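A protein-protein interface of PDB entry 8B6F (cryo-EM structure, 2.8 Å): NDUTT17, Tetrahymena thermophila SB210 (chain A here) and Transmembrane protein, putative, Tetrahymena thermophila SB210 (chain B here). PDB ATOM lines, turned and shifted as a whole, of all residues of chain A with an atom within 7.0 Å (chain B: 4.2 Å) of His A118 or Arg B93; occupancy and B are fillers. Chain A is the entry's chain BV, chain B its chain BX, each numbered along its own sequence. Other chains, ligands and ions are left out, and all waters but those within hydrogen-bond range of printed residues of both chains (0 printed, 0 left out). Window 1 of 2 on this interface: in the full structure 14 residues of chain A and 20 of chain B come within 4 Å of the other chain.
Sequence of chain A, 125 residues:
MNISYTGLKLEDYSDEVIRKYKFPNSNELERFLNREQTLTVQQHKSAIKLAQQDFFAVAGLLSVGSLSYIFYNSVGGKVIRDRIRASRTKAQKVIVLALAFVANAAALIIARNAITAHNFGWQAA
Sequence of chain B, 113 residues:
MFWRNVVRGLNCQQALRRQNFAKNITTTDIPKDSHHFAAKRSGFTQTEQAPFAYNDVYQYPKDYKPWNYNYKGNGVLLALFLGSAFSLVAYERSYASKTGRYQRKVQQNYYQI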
ATOM      1  N   ARG A 112     -24.788 -37.750 -20.348  1.00  0.00           N
ATOM      2  CA  ARG A 112     -25.391 -36.537 -20.891  1.00  0.00           C
ATOM      3  C   ARG A 112     -24.644 -36.045 -22.122  1.00  0.00           C
ATOM      4  O   ARG A 112     -25.255 -35.470 -23.028  1.00  0.00           O
ATOM      5  CB  ARG A 112     -25.423 -35.450 -19.812  1.00  0.00           C
ATOM      6  CG  ARG A 112     -25.905 -34.083 -20.284  1.00  0.00           C
ATOM      7  CD  ARG A 112     -27.313 -34.151 -20.845  1.00  0.00           C
ATOM      8  NE  ARG A 112     -27.908 -32.833 -21.029  1.00  0.00           N
ATOM      9  CZ  ARG A 112     -28.495 -32.131 -20.070  1.00  0.00           C
ATOM     10  NH1 ARG A 112     -28.569 -32.581 -18.829  1.00  0.00           N
ATOM     11  NH2 ARG A 112     -29.025 -30.948 -20.365  1.00  0.00           N
ATOM     12  N   ASN A 113     -23.330 -36.255 -22.167  1.00  0.00           N
ATOM     13  CA  ASN A 113     -22.530 -35.747 -23.275  1.00  0.00           C
ATOM     14  C   ASN A 113     -23.012 -36.298 -24.610  1.00  0.00           C
ATOM     15  O   ASN A 113     -23.074 -35.569 -25.606  1.00  0.00           O
ATOM     16  CB  ASN A 113     -21.062 -36.105 -23.051  1.00  0.00           C
ATOM     17  CG  ASN A 113     -20.245 -36.028 -24.321  1.00  0.00           C
ATOM     18  OD1 ASN A 113     -20.417 -35.117 -25.129  1.00  0.00           O
ATOM     19  ND2 ASN A 113     -19.356 -36.997 -24.512  1.00  0.00           N
ATOM     20  N   ALA A 114     -23.347 -37.586 -24.653  1.00  0.00           N
ATOM     21  CA  ALA A 114     -23.739 -38.209 -25.912  1.00  0.00           C
ATOM     22  C   ALA A 114     -25.028 -37.608 -26.461  1.00  0.00           C
ATOM     23  O   ALA A 114     -25.109 -37.265 -27.646  1.00  0.00           O
ATOM     24  CB  ALA A 114     -23.893 -39.712 -25.715  1.00  0.00           C
ATOM     25  N   ILE A 115     -26.052 -37.480 -25.617  1.00  0.00           N
ATOM     26  CA  ILE A 115     -27.315 -36.925 -26.091  1.00  0.00           C
ATOM     27  C   ILE A 115     -27.160 -35.455 -26.462  1.00  0.00           C
ATOM     28  O   ILE A 115     -27.799 -34.980 -27.407  1.00  0.00           O
ATOM     29  CB  ILE A 115     -28.424 -37.139 -25.042  1.00  0.00           C
ATOM     30  CG1 ILE A 115     -28.093 -36.417 -23.732  1.00  0.00           C
ATOM     31  CG2 ILE A 115     -28.626 -38.630 -24.803  1.00  0.00           C
ATOM     32  CD1 ILE A 115     -29.183 -36.528 -22.676  1.00  0.00           C
ATOM     33  N   THR A 116     -26.321 -34.714 -25.742  1.00  0.00           N
ATOM     34  CA  THR A 116     -26.088 -33.305 -26.049  1.00  0.00           C
ATOM     35  C   THR A 116     -25.057 -33.204 -27.166  1.00  0.00           C
ATOM     36  O   THR A 116     -23.870 -33.465 -26.951  1.00  0.00           O
ATOM     37  CB  THR A 116     -25.615 -32.552 -24.809  1.00  0.00           C
ATOM     38  OG1 THR A 116     -24.782 -33.405 -24.012  1.00  0.00           O
ATOM     39  CG2 THR A 116     -26.799 -32.081 -23.990  1.00  0.00           C
ATOM     40  N   ALA A 117     -25.509 -32.815 -28.354  1.00  0.00           N
ATOM     41  CA  ALA A 117     -24.630 -32.677 -29.512  1.00  0.00           C
ATOM     42  C   ALA A 117     -24.173 -31.225 -29.639  1.00  0.00           C
ATOM     43  O   ALA A 117     -24.621 -30.461 -30.496  1.00  0.00           O
ATOM     44  CB  ALA A 117     -25.341 -33.159 -30.772  1.00  0.00           C
ATOM     45  N   HIS A 118     -23.254 -30.852 -28.747  1.00  0.00           N
ATOM     46  CA  HIS A 118     -22.701 -29.505 -28.767  1.00  0.00           C
ATOM     47  C   HIS A 118     -21.676 -29.324 -29.879  1.00  0.00           C
ATOM     48  O   HIS A 118     -21.568 -28.230 -30.443  1.00  0.00           O
ATOM     49  CB  HIS A 118     -22.054 -29.183 -27.419  1.00  0.00           C
ATOM     50  CG  HIS A 118     -23.012 -29.206 -26.269  1.00  0.00           C
ATOM     51  ND1 HIS A 118     -24.363 -28.980 -26.418  1.00  0.00           N
ATOM     52  CD2 HIS A 118     -22.812 -29.431 -24.949  1.00  0.00           C
ATOM     53  CE1 HIS A 118     -24.954 -29.061 -25.240  1.00  0.00           C
ATOM     54  NE2 HIS A 118     -24.037 -29.334 -24.332  1.00  0.00           N
ATOM     55  N   ASN A 119     -20.923 -30.374 -30.207  1.00  0.00           N
ATOM     56  CA  ASN A 119     -19.843 -30.280 -31.190  1.00  0.00           C
ATOM     57  C   ASN A 119     -20.425 -30.383 -32.599  1.00  0.00           C
ATOM     58  O   ASN A 119     -20.199 -31.338 -33.345  1.00  0.00           O
ATOM     59  CB  ASN A 119     -18.801 -31.357 -30.933  1.00  0.00           C
ATOM     60  CG  ASN A 119     -18.192 -31.257 -29.550  1.00  0.00           C
ATOM     61  OD1 ASN A 119     -17.236 -30.512 -29.333  1.00  0.00           O
ATOM     62  ND2 ASN A 119     -18.745 -32.008 -28.605  1.00  0.00           N
ATOM     63  N   PHE A 120     -21.197 -29.362 -32.956  1.00  0.00           N
ATOM     64  CA  PHE A 120     -21.762 -29.213 -34.289  1.00  0.00           C
ATOM     65  C   PHE A 120     -21.189 -27.942 -34.895  1.00  0.00           C
ATOM     66  O   PHE A 120     -21.188 -26.891 -34.249  1.00  0.00           O
ATOM     67  CB  PHE A 120     -23.289 -29.156 -34.231  1.00  0.00           C
ATOM     68  CG  PHE A 120     -23.959 -29.430 -35.544  1.00  0.00           C
ATOM     69  CD1 PHE A 120     -24.220 -30.729 -35.946  1.00  0.00           C
ATOM     70  CD2 PHE A 120     -24.346 -28.391 -36.368  1.00  0.00           C
ATOM     71  CE1 PHE A 120     -24.841 -30.982 -37.150  1.00  0.00           C
ATOM     72  CE2 PHE A 120     -24.966 -28.638 -37.571  1.00  0.00           C
ATOM     73  CZ  PHE A 120     -25.213 -29.933 -37.962  1.00  0.00           C
ATOM     74  N   GLY A 121     -20.698 -28.036 -36.129  1.00  0.00           N
ATOM     75  CA  GLY A 121     -19.946 -26.934 -36.703  1.00  0.00           C
ATOM     76  C   GLY A 121     -20.782 -25.751 -37.142  1.00  0.00           C
ATOM     77  O   GLY A 121     -20.209 -24.725 -37.526  1.00  0.00           O
ATOM     78  N   GLN A 123     -22.605 -23.766 -35.387  1.00  0.00           N
ATOM     79  CA  GLN A 123     -22.751 -22.696 -34.410  1.00  0.00           C
ATOM     80  C   GLN A 123     -22.241 -21.391 -35.005  1.00  0.00           C
ATOM     81  O   GLN A 123     -21.045 -21.248 -35.268  1.00  0.00           O
ATOM     82  CB  GLN A 123     -21.991 -23.021 -33.121  1.00  0.00           C
ATOM     83  CG  GLN A 123     -22.272 -24.398 -32.543  1.00  0.00           C
ATOM     84  CD  GLN A 123     -23.741 -24.649 -32.288  1.00  0.00           C
ATOM     85  OE1 GLN A 123     -24.542 -23.718 -32.231  1.00  0.00           O
ATOM     86  NE2 GLN A 123     -24.105 -25.916 -32.134  1.00  0.00           N
ATOM     87  N   VAL B  89     -26.431 -25.380 -16.291  1.00  0.00           N
ATOM     88  CA  VAL B  89     -25.444 -25.028 -17.306  1.00  0.00           C
ATOM     89  C   VAL B  89     -25.607 -25.913 -18.534  1.00  0.00           C
ATOM     90  O   VAL B  89     -25.431 -25.460 -19.670  1.00  0.00           O
ATOM     91  CB  VAL B  89     -24.020 -25.107 -16.730  1.00  0.00           C
ATOM     92  CG1 VAL B  89     -23.664 -26.533 -16.339  1.00  0.00           C
ATOM     93  CG2 VAL B  89     -23.033 -24.558 -17.728  1.00  0.00           C
ATOM     94  N   ALA B  90     -25.939 -27.187 -18.326  1.00  0.00           N
ATOM     95  CA  ALA B  90     -26.169 -28.081 -19.455  1.00  0.00           C
ATOM     96  C   ALA B  90     -27.361 -27.621 -20.280  1.00  0.00           C
ATOM     97  O   ALA B  90     -27.325 -27.674 -21.515  1.00  0.00           O
ATOM     98  CB  ALA B  90     -26.379 -29.512 -18.956  1.00  0.00           C
ATOM     99  N   TYR B  91     -28.431 -27.172 -19.622  1.00  0.00           N
ATOM    100  CA  TYR B  91     -29.569 -26.648 -20.366  1.00  0.00           C
ATOM    101  C   TYR B  91     -29.196 -25.381 -21.124  1.00  0.00           C
ATOM    102  O   TYR B  91     -29.635 -25.185 -22.262  1.00  0.00           O
ATOM    103  CB  TYR B  91     -30.747 -26.369 -19.438  1.00  0.00           C
ATOM    104  CG  TYR B  91     -31.917 -25.782 -20.190  1.00  0.00           C
ATOM    105  CD1 TYR B  91     -32.772 -26.595 -20.918  1.00  0.00           C
ATOM    106  CD2 TYR B  91     -32.144 -24.413 -20.201  1.00  0.00           C
ATOM    107  CE1 TYR B  91     -33.830 -26.065 -21.623  1.00  0.00           C
ATOM    108  CE2 TYR B  91     -33.201 -23.872 -20.905  1.00  0.00           C
ATOM    109  CZ  TYR B  91     -34.040 -24.705 -21.613  1.00  0.00           C
ATOM    110  OH  TYR B  91     -35.096 -24.179 -22.317  1.00  0.00           O
ATOM    111  N   GLU B  92     -28.392 -24.509 -20.514  1.00  0.00           N
ATOM    112  CA  GLU B  92     -27.934 -23.319 -21.222  1.00  0.00           C
ATOM    113  C   GLU B  92     -27.204 -23.704 -22.501  1.00  0.00           C
ATOM    114  O   GLU B  92     -27.480 -23.161 -23.577  1.00  0.00           O
ATOM    115  CB  GLU B  92     -27.025 -22.490 -20.317  1.00  0.00           C
ATOM    116  CG  GLU B  92     -27.724 -21.880 -19.117  1.00  0.00           C
ATOM    117  CD  GLU B  92     -28.649 -20.744 -19.496  1.00  0.00           C
ATOM    118  OE1 GLU B  92     -28.752 -20.433 -20.700  1.00  0.00           O
ATOM    119  OE2 GLU B  92     -29.275 -20.161 -18.588  1.00  0.00           O
ATOM    120  N   ARG B  93     -26.258 -24.637 -22.399  1.00  0.00           N
ATOM    121  CA  ARG B  93     -25.504 -25.057 -23.574  1.00  0.00           C
ATOM    122  C   ARG B  93     -26.415 -25.716 -24.601  1.00  0.00           C
ATOM    123  O   ARG B  93     -26.258 -25.507 -25.808  1.00  0.00           O
ATOM    124  CB  ARG B  93     -24.378 -26.003 -23.161  1.00  0.00           C
ATOM    125  CG  ARG B  93     -23.277 -26.145 -24.198  1.00  0.00           C
ATOM    126  CD  ARG B  93     -22.443 -24.880 -24.298  1.00  0.00           C
ATOM    127  NE  ARG B  93     -21.293 -25.056 -25.176  1.00  0.00           N
ATOM    128  CZ  ARG B  93     -21.307 -24.865 -26.488  1.00  0.00           C
ATOM    129  NH1 ARG B  93     -22.408 -24.492 -27.123  1.00  0.00           N
ATOM    130  NH2 ARG B  93     -20.188 -25.048 -27.182  1.00  0.00           N
ATOM    131  N   SER B  94     -27.372 -26.521 -24.137  1.00  0.00           N
ATOM    132  CA  SER B  94     -28.294 -27.180 -25.055  1.00  0.00           C
ATOM    133  C   SER B  94     -29.142 -26.167 -25.811  1.00  0.00           C
ATOM    134  O   SER B  94     -29.356 -26.305 -27.021  1.00  0.00           O
ATOM    135  CB  SER B  94     -29.190 -28.157 -24.292  1.00  0.00           C
ATOM    136  OG  SER B  94     -28.430 -29.190 -23.693  1.00  0.00           O
ATOM    137  N   TYR B  95     -29.638 -25.141 -25.117  1.00  0.00           N
ATOM    138  CA  TYR B  95     -30.422 -24.112 -25.790  1.00  0.00           C
ATOM    139  C   TYR B  95     -29.582 -23.362 -26.812  1.00  0.00           C
ATOM    140  O   TYR B  95     -30.053 -23.066 -27.915  1.00  0.00           O
ATOM    141  CB  TYR B  95     -31.011 -23.141 -24.770  1.00  0.00           C
ATOM    142  CG  TYR B  95     -31.740 -21.984 -25.408  1.00  0.00           C
ATOM    143  CD1 TYR B  95     -33.024 -22.141 -25.910  1.00  0.00           C
ATOM    144  CD2 TYR B  95     -31.143 -20.736 -25.511  1.00  0.00           C
ATOM    145  CE1 TYR B  95     -33.692 -21.086 -26.497  1.00  0.00           C
ATOM    146  CE2 TYR B  95     -31.802 -19.676 -26.096  1.00  0.00           C
ATOM    147  CZ  TYR B  95     -33.077 -19.858 -26.586  1.00  0.00           C
ATOM    148  OH  TYR B  95     -33.740 -18.805 -27.169  1.00  0.00           O
ATOM    149  N   ALA B  96     -28.333 -23.049 -26.470  1.00  0.00           N
ATOM    150  CA  ALA B  96     -27.459 -22.395 -27.435  1.00  0.00           C
ATOM    151  C   ALA B  96     -27.267 -23.269 -28.668  1.00  0.00           C
ATOM    152  O   ALA B  96     -27.306 -22.776 -29.800  1.00  0.00           O
ATOM    153  CB  ALA B  96     -26.115 -22.070 -26.787  1.00  0.00           C
ATOM    154  N   SER B  97     -27.050 -24.569 -28.467  1.00  0.00           N
ATOM    155  CA  SER B  97     -26.870 -25.473 -29.598  1.00  0.00           C
ATOM    156  C   SER B  97     -28.128 -25.549 -30.455  1.00  0.00           C
ATOM    157  O   SER B  97     -28.048 -25.564 -31.688  1.00  0.00           O
ATOM    158  CB  SER B  97     -26.480 -26.863 -29.099  1.00  0.00           C
ATOM    159  OG  SER B  97     -25.245 -26.822 -28.410  1.00  0.00           O
ATOM    160  N   TYR B 102     -22.986 -20.154 -30.283  1.00  0.00           N
ATOM    161  CA  TYR B 102     -22.035 -20.566 -29.259  1.00  0.00           C
ATOM    162  C   TYR B 102     -22.500 -20.195 -27.860  1.00  0.00           C
ATOM    163  O   TYR B 102     -22.003 -20.764 -26.884  1.00  0.00           O
ATOM    164  CB  TYR B 102     -20.665 -19.941 -29.525  1.00  0.00           C
ATOM    165  CG  TYR B 102     -19.970 -20.488 -30.749  1.00  0.00           C
ATOM    166  CD1 TYR B 102     -19.410 -21.759 -30.743  1.00  0.00           C
ATOM    167  CD2 TYR B 102     -19.861 -19.729 -31.906  1.00  0.00           C
ATOM    168  CE1 TYR B 102     -18.770 -22.263 -31.858  1.00  0.00           C
ATOM    169  CE2 TYR B 102     -19.223 -20.223 -33.026  1.00  0.00           C
ATOM    170  CZ  TYR B 102     -18.679 -21.489 -32.996  1.00  0.00           C
ATOM    171  OH  TYR B 102     -18.042 -21.987 -34.108  1.00  0.00           O
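The side-chain hydroxyl of Thr A116 lies within hydrogen-bond range of the backbone carbonyl oxygen of Asn A113 (3.2 Å). The backbone carbonyl oxygen of Ala B90 is in hydrogen-bond range of the side-chain hydroxyl of Ser B94 (2.9 Å). OG of Ser B97 sits at hydrogen-bond distance from O of Arg B93, at 3.1 Å.
Of the 11 printed residues of chain A, 4 touch a printed residue of chain B. Hydrophobic or aromatic side chains of chain A that line the printed part of chain B: His A118. Among the printed residues, 10 pairs touch across the chains.
Among the printed residues, pairs that only touch across the chains: His A118 with Arg B93 (3.3 Å), Arg A112 with Ala B90 (3.3 Å), Thr A116 with Ser B94 (3.3 Å), His A118 with Ser B94 (3.7 Å), Gln A123 with Ser B97 (3.8 Å), Gln A123 with Ala B96 (3.8 Å), Arg A112 with Ser B94 (3.8 Å) and Arg A112 with Tyr B91 (3.9 Å).
A ring nitrogen (ND1) of His A118 is in hydrogen-bond range of the side-chain hydroxyl (OG) of Ser B97 (3.1 Å). The backbone carbonyl oxygen of Gln A123 lies close to the side-chain hydroxyl of Tyr B102, at 3.3 Å.
Ile A115 touches none of the printed residues of chain B. Of chain B, only Arg B93 (3.3 Å), Ser B94 (3.7 Å) and Ser B97 (3.1 Å) come within 4 Å of His A118. Phe A120 touches none of the printed residues of chain B. Of the printed residues of chain B, Gln A123 touches Ala B96 (3.8 Å), Ser B97 (3.8 Å) and Tyr B102 (3.1 Å). Printed residues of chain A within 4 Å of Ala B90: Arg A112 (3.3 Å). Printed residues of chain A within 4 Å of Ser B94: Arg A112 (3.8 Å), Thr A116 (3.3 Å) and His A118 (3.7 Å). The nearest printed residue of chain B that does not touch His A118 is Ala B90 (4.6 Å). The nearest printed residue of chain A that does not touch Ala B90 is His A118 (4.6 Å).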
